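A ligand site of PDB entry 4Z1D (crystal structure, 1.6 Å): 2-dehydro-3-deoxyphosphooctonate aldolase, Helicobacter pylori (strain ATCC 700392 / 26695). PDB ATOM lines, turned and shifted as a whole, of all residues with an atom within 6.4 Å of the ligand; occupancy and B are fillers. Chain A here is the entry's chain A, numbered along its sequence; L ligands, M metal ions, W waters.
Asp 87 touches the ligand. Pro 107 touches the ligand (CA to O4, 3.2 Å). CE1 of His 204 touches O2 of the ligand (3.4 Å). Phe 239 touches the ligand (CZ to O2, 3.4 Å). Glu 241 touches the ligand. Hydrophobic or aromatic side chains that line the ligand: Pro 107, Ala 108, His 204 and Phe 239. Within 4 Å of the ligand: Lys 47, Ser 49, Lys 52, Asp 87, Gln 105, Pro 107, Ala 108, Lys 130, Arg 173, His 204, Phe 239 and Glu 241. Along chain A the residues within 4 Å of the ligand span positions 47 to 241.
OG of Ser 49 is in hydrogen-bond range of O1 of the ligand, 3.2 Å away. The guanidinium group (NH2) of Arg 173 lies within salt-bridge range of an oxygen (O6) of the ligand. The side-chain amino group (NZ) of Lys 52 lies within salt-bridge range of an oxygen (O1) of the ligand, at 3.1 Å. NE2 of Gln 105 lies within hydrogen-bond range of O2 of the ligand. O5 of the ligand lies within salt-bridge range of NZ of Lys 130, at 2.8 Å. NZ of Lys 47 is in salt-bridge range of O1 of the ligand. The backbone NH (N) of Ala 108 lies within hydrogen-bond range of an oxygen (O4) of the ligand, 2.9 Å away.
Water W1 bridges O6 of the ligand (2.7 Å) and NE2 of Gln 133 (3.2 Å). Water W3 lies within hydrogen-bond range of O4 of the ligand (2.8 Å), N of Phe 109 (3.2 Å) and N of Ala 108 (3.3 Å). Water W5 lies within hydrogen-bond range of the side-chain amide nitrogen (NE2) of Gln 105, the side-chain carboxylate (OD2) of Asp 87 and an oxygen (O4) of the ligand.
OD2 of Asp 201 is in hydrogen-bond range of ND1 of His 204. The side-chain hydroxyl (OG) of Ser 49 lies within hydrogen-bond range of the backbone carbonyl oxygen (O) of Cys 18 (3.1 Å). The guanidinium group (NH1) of Arg 173 sits at hydrogen-bond distance from the backbone carbonyl oxygen (O) of His 204 (2.9 Å). The side-chain hydroxyl of Ser 49 lies within hydrogen-bond range of the side-chain carboxylate of Asp 87. The guanidinium group (NH1) of Arg 173 sits close to the side-chain amide nitrogen (NE2) of Gln 133 (3.4 Å). The side-chain amino group of Lys 47 lies within hydrogen-bond range of the backbone carbonyl oxygen of Cys 18 (3.1 Å). The backbone carbonyl oxygen (O) of Ile 106 is in hydrogen-bond range of the backbone NH (N) of Lys 130. The side-chain amino group of Lys 130 is in salt-bridge range of the side-chain carboxylate of Asp 201 (2.8 Å).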
ATOM      1  N   CYS A  18       8.987  18.284 -11.511  1.00  0.00           N
ATOM      2  CA  CYS A  18       9.565  17.467 -12.577  1.00  0.00           C
ATOM      3  C   CYS A  18       8.767  16.199 -12.762  1.00  0.00           C
ATOM      4  O   CYS A  18       8.378  15.853 -13.881  1.00  0.00           O
ATOM      5  CB  CYS A  18      11.013  17.137 -12.252  1.00  0.00           C
ATOM      6  SG  CYS A  18      11.934  16.450 -13.634  1.00  0.00           S
ATOM      7  N   LYS A  47       2.522  21.486 -15.081  1.00  0.00           N
ATOM      8  CA  LYS A  47       3.339  20.408 -15.626  1.00  0.00           C
ATOM      9  C   LYS A  47       3.718  19.383 -14.566  1.00  0.00           C
ATOM     10  O   LYS A  47       4.097  19.741 -13.464  1.00  0.00           O
ATOM     11  CB  LYS A  47       4.639  20.996 -16.223  1.00  0.00           C
ATOM     12  CG  LYS A  47       5.533  20.017 -16.973  1.00  0.00           C
ATOM     13  CD  LYS A  47       6.650  19.364 -16.156  1.00  0.00           C
ATOM     14  CE  LYS A  47       7.389  18.322 -16.990  1.00  0.00           C
ATOM     15  NZ  LYS A  47       8.599  17.731 -16.347  1.00  0.00           N
ATOM     16  N   SER A  49       5.555  15.179 -14.996  1.00  0.00           N
ATOM     17  CA  SER A  49       5.787  13.941 -15.746  1.00  0.00           C
ATOM     18  C   SER A  49       5.226  12.750 -14.983  1.00  0.00           C
ATOM     19  O   SER A  49       5.444  12.612 -13.785  1.00  0.00           O
ATOM     20  CB  SER A  49       7.276  13.731 -15.967  1.00  0.00           C
ATOM     21  OG  SER A  49       7.838  14.783 -16.728  1.00  0.00           O
ATOM     22  N   ASP A  51       6.166   9.723 -16.009  1.00  0.00           N
ATOM     23  CA  ASP A  51       7.295   8.796 -16.139  1.00  0.00           C
ATOM     24  C   ASP A  51       8.587   9.563 -16.404  1.00  0.00           C
ATOM     25  O   ASP A  51       8.623  10.432 -17.261  1.00  0.00           O
ATOM     26  CB  ASP A  51       7.059   7.825 -17.297  1.00  0.00           C
ATOM     27  CG  ASP A  51       8.204   6.820 -17.458  1.00  0.00           C
ATOM     28  OD1 ASP A  51       8.719   6.330 -16.438  1.00  0.00           O
ATOM     29  OD2 ASP A  51       8.573   6.521 -18.610  1.00  0.00           O
ATOM     30  N   LYS A  52       9.638   9.208 -15.666  1.00  0.00           N
ATOM     31  CA  LYS A  52      10.995   9.633 -15.976  1.00  0.00           C
ATOM     32  C   LYS A  52      11.688   8.415 -16.577  1.00  0.00           C
ATOM     33  O   LYS A  52      12.035   7.472 -15.880  1.00  0.00           O
ATOM     34  CB  LYS A  52      11.726  10.113 -14.723  1.00  0.00           C
ATOM     35  CG  LYS A  52      10.963  11.156 -13.904  1.00  0.00           C
ATOM     36  CD  LYS A  52      10.431  12.316 -14.716  1.00  0.00           C
ATOM     37  CE  LYS A  52      11.530  13.173 -15.318  1.00  0.00           C
ATOM     38  NZ  LYS A  52      10.960  14.324 -16.071  1.00  0.00           N
ATOM     39  N   LEU A  85       0.105  20.076 -18.744  1.00  0.00           N
ATOM     40  CA  LEU A  85       1.133  19.573 -19.660  1.00  0.00           C
ATOM     41  C   LEU A  85       1.778  18.315 -19.102  1.00  0.00           C
ATOM     42  O   LEU A  85       2.169  18.279 -17.929  1.00  0.00           O
ATOM     43  CB  LEU A  85       2.224  20.629 -19.916  1.00  0.00           C
ATOM     44  CG  LEU A  85       3.300  20.206 -20.930  1.00  0.00           C
ATOM     45  CD1 LEU A  85       3.884  21.424 -21.619  1.00  0.00           C
ATOM     46  CD2 LEU A  85       4.417  19.380 -20.296  1.00  0.00           C
ATOM     47  N   ASP A  87       4.576  14.946 -20.621  1.00  0.00           N
ATOM     48  CA  ASP A  87       5.360  14.426 -21.741  1.00  0.00           C
ATOM     49  C   ASP A  87       5.015  12.974 -21.997  1.00  0.00           C
ATOM     50  O   ASP A  87       4.644  12.239 -21.094  1.00  0.00           O
ATOM     51  CB  ASP A  87       6.865  14.632 -21.543  1.00  0.00           C
ATOM     52  CG  ASP A  87       7.416  14.064 -20.235  1.00  0.00           C
ATOM     53  OD1 ASP A  87       6.710  14.028 -19.208  1.00  0.00           O
ATOM     54  OD2 ASP A  87       8.604  13.691 -20.250  1.00  0.00           O
ATOM     55  N   HIS A  89       6.253   9.262 -24.180  1.00  0.00           N
ATOM     56  CA  HIS A  89       7.507   8.531 -24.410  1.00  0.00           C
ATOM     57  C   HIS A  89       7.403   7.384 -25.424  1.00  0.00           C
ATOM     58  O   HIS A  89       8.418   6.952 -25.958  1.00  0.00           O
ATOM     59  CB  HIS A  89       7.990   7.939 -23.092  1.00  0.00           C
ATOM     60  CG  HIS A  89       7.965   8.915 -21.952  1.00  0.00           C
ATOM     61  ND1 HIS A  89       9.004   9.776 -21.685  1.00  0.00           N
ATOM     62  CD2 HIS A  89       6.995   9.195 -21.042  1.00  0.00           C
ATOM     63  CE1 HIS A  89       8.691  10.526 -20.636  1.00  0.00           C
ATOM     64  NE2 HIS A  89       7.473  10.189 -20.233  1.00  0.00           N
ATOM     65  N   GLN A 105       3.976  16.937 -24.624  1.00  0.00           N
ATOM     66  CA  GLN A 105       5.357  17.299 -24.889  1.00  0.00           C
ATOM     67  C   GLN A 105       6.133  16.121 -25.447  1.00  0.00           C
ATOM     68  O   GLN A 105       6.059  15.015 -24.914  1.00  0.00           O
ATOM     69  CB  GLN A 105       6.001  17.800 -23.613  1.00  0.00           C
ATOM     70  CG  GLN A 105       7.475  18.143 -23.756  1.00  0.00           C
ATOM     71  CD  GLN A 105       7.956  18.822 -22.513  1.00  0.00           C
ATOM     72  OE1 GLN A 105       7.629  19.976 -22.273  1.00  0.00           O
ATOM     73  NE2 GLN A 105       8.710  18.097 -21.687  1.00  0.00           N
ATOM     74  N   ILE A 106       6.879  16.392 -26.527  1.00  0.00           N
ATOM     75  CA  ILE A 106       7.797  15.443 -27.139  1.00  0.00           C
ATOM     76  C   ILE A 106       9.160  15.648 -26.495  1.00  0.00           C
ATOM     77  O   ILE A 106       9.730  16.727 -26.605  1.00  0.00           O
ATOM     78  CB  ILE A 106       7.946  15.708 -28.669  1.00  0.00           C
ATOM     79  CG1 ILE A 106       6.577  15.718 -29.361  1.00  0.00           C
ATOM     80  CG2 ILE A 106       8.889  14.686 -29.313  1.00  0.00           C
ATOM     81  CD1 ILE A 106       5.924  14.370 -29.468  1.00  0.00           C
ATOM     82  N   PRO A 107       9.703  14.617 -25.815  1.00  0.00           N
ATOM     83  CA  PRO A 107      11.001  14.777 -25.135  1.00  0.00           C
ATOM     84  C   PRO A 107      12.134  15.081 -26.101  1.00  0.00           C
ATOM     85  O   PRO A 107      12.077  14.710 -27.263  1.00  0.00           O
ATOM     86  CB  PRO A 107      11.238  13.411 -24.483  1.00  0.00           C
ATOM     87  CG  PRO A 107       9.891  12.779 -24.386  1.00  0.00           C
ATOM     88  CD  PRO A 107       9.113  13.298 -25.563  1.00  0.00           C
ATOM     89  N   ALA A 108      13.166  15.747 -25.582  1.00  0.00           N
ATOM     90  CA  ALA A 108      14.287  16.223 -26.384  1.00  0.00           C
ATOM     91  C   ALA A 108      14.977  15.115 -27.159  1.00  0.00           C
ATOM     92  O   ALA A 108      15.325  15.299 -28.331  1.00  0.00           O
ATOM     93  CB  ALA A 108      15.288  16.949 -25.490  1.00  0.00           C
ATOM     94  N   PHE A 109      15.165  13.958 -26.515  1.00  0.00           N
ATOM     95  CA  PHE A 109      15.802  12.813 -27.183  1.00  0.00           C
ATOM     96  C   PHE A 109      14.957  12.227 -28.320  1.00  0.00           C
ATOM     97  O   PHE A 109      15.499  11.548 -29.203  1.00  0.00           O
ATOM     98  CB  PHE A 109      16.108  11.676 -26.194  1.00  0.00           C
ATOM     99  CG  PHE A 109      17.172  11.993 -25.161  1.00  0.00           C
ATOM    100  CD1 PHE A 109      18.141  12.965 -25.377  1.00  0.00           C
ATOM    101  CD2 PHE A 109      17.219  11.243 -23.983  1.00  0.00           C
ATOM    102  CE1 PHE A 109      19.111  13.217 -24.411  1.00  0.00           C
ATOM    103  CE2 PHE A 109      18.192  11.490 -23.029  1.00  0.00           C
ATOM    104  CZ  PHE A 109      19.137  12.479 -23.237  1.00  0.00           C
ATOM    105  N   LYS A 130      10.378  19.577 -27.588  1.00  0.00           N
ATOM    106  CA  LYS A 130      11.685  19.925 -26.995  1.00  0.00           C
ATOM    107  C   LYS A 130      12.774  19.761 -28.041  1.00  0.00           C
ATOM    108  O   LYS A 130      12.862  18.704 -28.690  1.00  0.00           O
ATOM    109  CB  LYS A 130      11.998  19.043 -25.787  1.00  0.00           C
ATOM    110  CG  LYS A 130      11.155  19.242 -24.514  1.00  0.00           C
ATOM    111  CD  LYS A 130      11.465  20.572 -23.838  1.00  0.00           C
ATOM    112  CE  LYS A 130      11.065  20.627 -22.375  1.00  0.00           C
ATOM    113  NZ  LYS A 130      12.019  19.954 -21.456  1.00  0.00           N
ATOM    114  N   LYS A 131      13.599  20.783 -28.248  1.00  0.00           N
ATOM    115  CA  LYS A 131      14.758  20.637 -29.137  1.00  0.00           C
ATOM    116  C   LYS A 131      15.847  19.764 -28.497  1.00  0.00           C
ATOM    117  O   LYS A 131      16.354  20.078 -27.420  1.00  0.00           O
ATOM    118  CB  LYS A 131      15.351  21.991 -29.517  1.00  0.00           C
ATOM    119  CG  LYS A 131      16.676  21.882 -30.267  1.00  0.00           C
ATOM    120  CD  LYS A 131      17.073  23.136 -31.024  1.00  0.00           C
ATOM    121  CE  LYS A 131      17.278  24.322 -30.106  1.00  0.00           C
ATOM    122  NZ  LYS A 131      18.345  24.107 -29.092  1.00  0.00           N
ATOM    123  N   GLN A 133      19.402  18.189 -27.520  1.00  0.00           N
ATOM    124  CA  GLN A 133      20.672  18.817 -27.152  1.00  0.00           C
ATOM    125  C   GLN A 133      21.677  18.710 -28.304  1.00  0.00           C
ATOM    126  O   GLN A 133      22.673  19.449 -28.346  1.00  0.00           O
ATOM    127  CB  GLN A 133      21.229  18.131 -25.891  1.00  0.00           C
ATOM    128  CG  GLN A 133      20.327  18.203 -24.653  1.00  0.00           C
ATOM    129  CD  GLN A 133      19.311  17.062 -24.546  1.00  0.00           C
ATOM    130  OE1 GLN A 133      18.819  16.541 -25.545  1.00  0.00           O
ATOM    131  NE2 GLN A 133      18.983  16.679 -23.307  1.00  0.00           N
ATOM    132  N   ARG A 173      15.966  24.029 -24.780  1.00  0.00           N
ATOM    133  CA  ARG A 173      16.434  23.490 -23.500  1.00  0.00           C
ATOM    134  C   ARG A 173      17.961  23.284 -23.447  1.00  0.00           C
ATOM    135  O   ARG A 173      18.465  22.515 -22.620  1.00  0.00           O
ATOM    136  CB  ARG A 173      15.699  22.178 -23.154  1.00  0.00           C
ATOM    137  CG  ARG A 173      15.947  20.989 -24.084  1.00  0.00           C
ATOM    138  CD  ARG A 173      16.199  19.720 -23.289  1.00  0.00           C
ATOM    139  NE  ARG A 173      17.474  19.757 -22.589  1.00  0.00           N
ATOM    140  CZ  ARG A 173      17.769  19.065 -21.493  1.00  0.00           C
ATOM    141  NH1 ARG A 173      18.960  19.224 -20.978  1.00  0.00           N
ATOM    142  NH2 ARG A 173      16.900  18.246 -20.910  1.00  0.00           N
ATOM    143  N   ASP A 201      12.819  26.579 -21.754  1.00  0.00           N
ATOM    144  CA  ASP A 201      12.930  25.720 -20.572  1.00  0.00           C
ATOM    145  C   ASP A 201      14.109  26.205 -19.725  1.00  0.00           C
ATOM    146  O   ASP A 201      15.276  25.973 -20.071  1.00  0.00           O
ATOM    147  CB  ASP A 201      13.098  24.252 -21.012  1.00  0.00           C
ATOM    148  CG  ASP A 201      13.307  23.286 -19.872  1.00  0.00           C
ATOM    149  OD1 ASP A 201      13.587  23.685 -18.720  1.00  0.00           O
ATOM    150  OD2 ASP A 201      13.215  22.064 -20.153  1.00  0.00           O
ATOM    151  N   HIS A 204      16.009  22.777 -17.281  1.00  0.00           N
ATOM    152  CA  HIS A 204      16.863  21.703 -17.770  1.00  0.00           C
ATOM    153  C   HIS A 204      18.019  22.195 -18.618  1.00  0.00           C
ATOM    154  O   HIS A 204      18.814  21.383 -19.072  1.00  0.00           O
ATOM    155  CB  HIS A 204      16.065  20.694 -18.579  1.00  0.00           C
ATOM    156  CG  HIS A 204      14.932  20.075 -17.825  1.00  0.00           C
ATOM    157  ND1 HIS A 204      13.622  20.258 -18.180  1.00  0.00           N
ATOM    158  CD2 HIS A 204      14.924  19.291 -16.727  1.00  0.00           C
ATOM    159  CE1 HIS A 204      12.835  19.604 -17.339  1.00  0.00           C
ATOM    160  NE2 HIS A 204      13.603  19.003 -16.448  1.00  0.00           N
ATOM    161  N   PHE A 239       9.032  27.755 -19.522  1.00  0.00           N
ATOM    162  CA  PHE A 239       8.877  26.461 -18.866  1.00  0.00           C
ATOM    163  C   PHE A 239       9.849  26.450 -17.684  1.00  0.00           C
ATOM    164  O   PHE A 239      11.049  26.658 -17.860  1.00  0.00           O
ATOM    165  CB  PHE A 239       9.190  25.363 -19.894  1.00  0.00           C
ATOM    166  CG  PHE A 239       9.215  23.959 -19.362  1.00  0.00           C
ATOM    167  CD1 PHE A 239      10.212  23.538 -18.471  1.00  0.00           C
ATOM    168  CD2 PHE A 239       8.293  23.018 -19.817  1.00  0.00           C
ATOM    169  CE1 PHE A 239      10.252  22.226 -18.027  1.00  0.00           C
ATOM    170  CE2 PHE A 239       8.348  21.703 -19.376  1.00  0.00           C
ATOM    171  CZ  PHE A 239       9.323  21.314 -18.474  1.00  0.00           C
ATOM    172  N   GLU A 241      10.362  24.310 -13.820  1.00  0.00           N
ATOM    173  CA  GLU A 241       9.895  23.391 -12.790  1.00  0.00           C
ATOM    174  C   GLU A 241      10.040  23.988 -11.390  1.00  0.00           C
ATOM    175  O   GLU A 241      11.007  24.696 -11.078  1.00  0.00           O
ATOM    176  CB  GLU A 241      10.588  22.040 -12.909  1.00  0.00           C
ATOM    177  CG  GLU A 241      10.223  21.362 -14.217  1.00  0.00           C
ATOM    178  CD  GLU A 241      10.989  20.086 -14.481  1.00  0.00           C
ATOM    179  OE1 GLU A 241      12.073  19.864 -13.879  1.00  0.00           O
ATOM    180  OE2 GLU A 241      10.512  19.296 -15.331  1.00  0.00           O
HETATM  181  C1  LIG L   1      10.798  17.110 -19.026  1.00  0.00           C
HETATM  182  O1  LIG L   1      10.217  16.520 -18.080  1.00  0.00           O
HETATM  183  O2  LIG L   1      10.515  18.287 -19.375  1.00  0.00           O
HETATM  184  C2  LIG L   1      11.856  16.439 -19.766  1.00  0.00           C
HETATM  185  C3  LIG L   1      12.126  15.160 -19.582  1.00  0.00           C
HETATM  186  O3  LIG L   1      12.560  17.269 -20.729  1.00  0.00           O
HETATM  187  P1  LIG L   1      13.606  16.808 -21.870  1.00  0.00           P
HETATM  188  O4  LIG L   1      12.902  15.766 -22.726  1.00  0.00           O
HETATM  189  O5  LIG L   1      13.810  18.136 -22.529  1.00  0.00           O
HETATM  190  O6  LIG L   1      14.775  16.272 -21.070  1.00  0.00           O
HETATM  191 ZN    ZN M   1      12.955  18.317 -14.538  1.00  0.00          ZN
HETATM  192  O   HOH W   1      16.759  14.772 -22.138  1.00  0.00           O
HETATM  193  O   HOH W   2      13.513  15.681 -16.549  1.00  0.00           O
HETATM  194  O   HOH W   3      14.498  13.540 -23.448  1.00  0.00           O
HETATM  195  O   HOH W   4      15.353  15.934 -18.509  1.00  0.00           O
HETATM  196  O   HOH W   5       9.997  15.538 -22.092  1.00  0.00           O
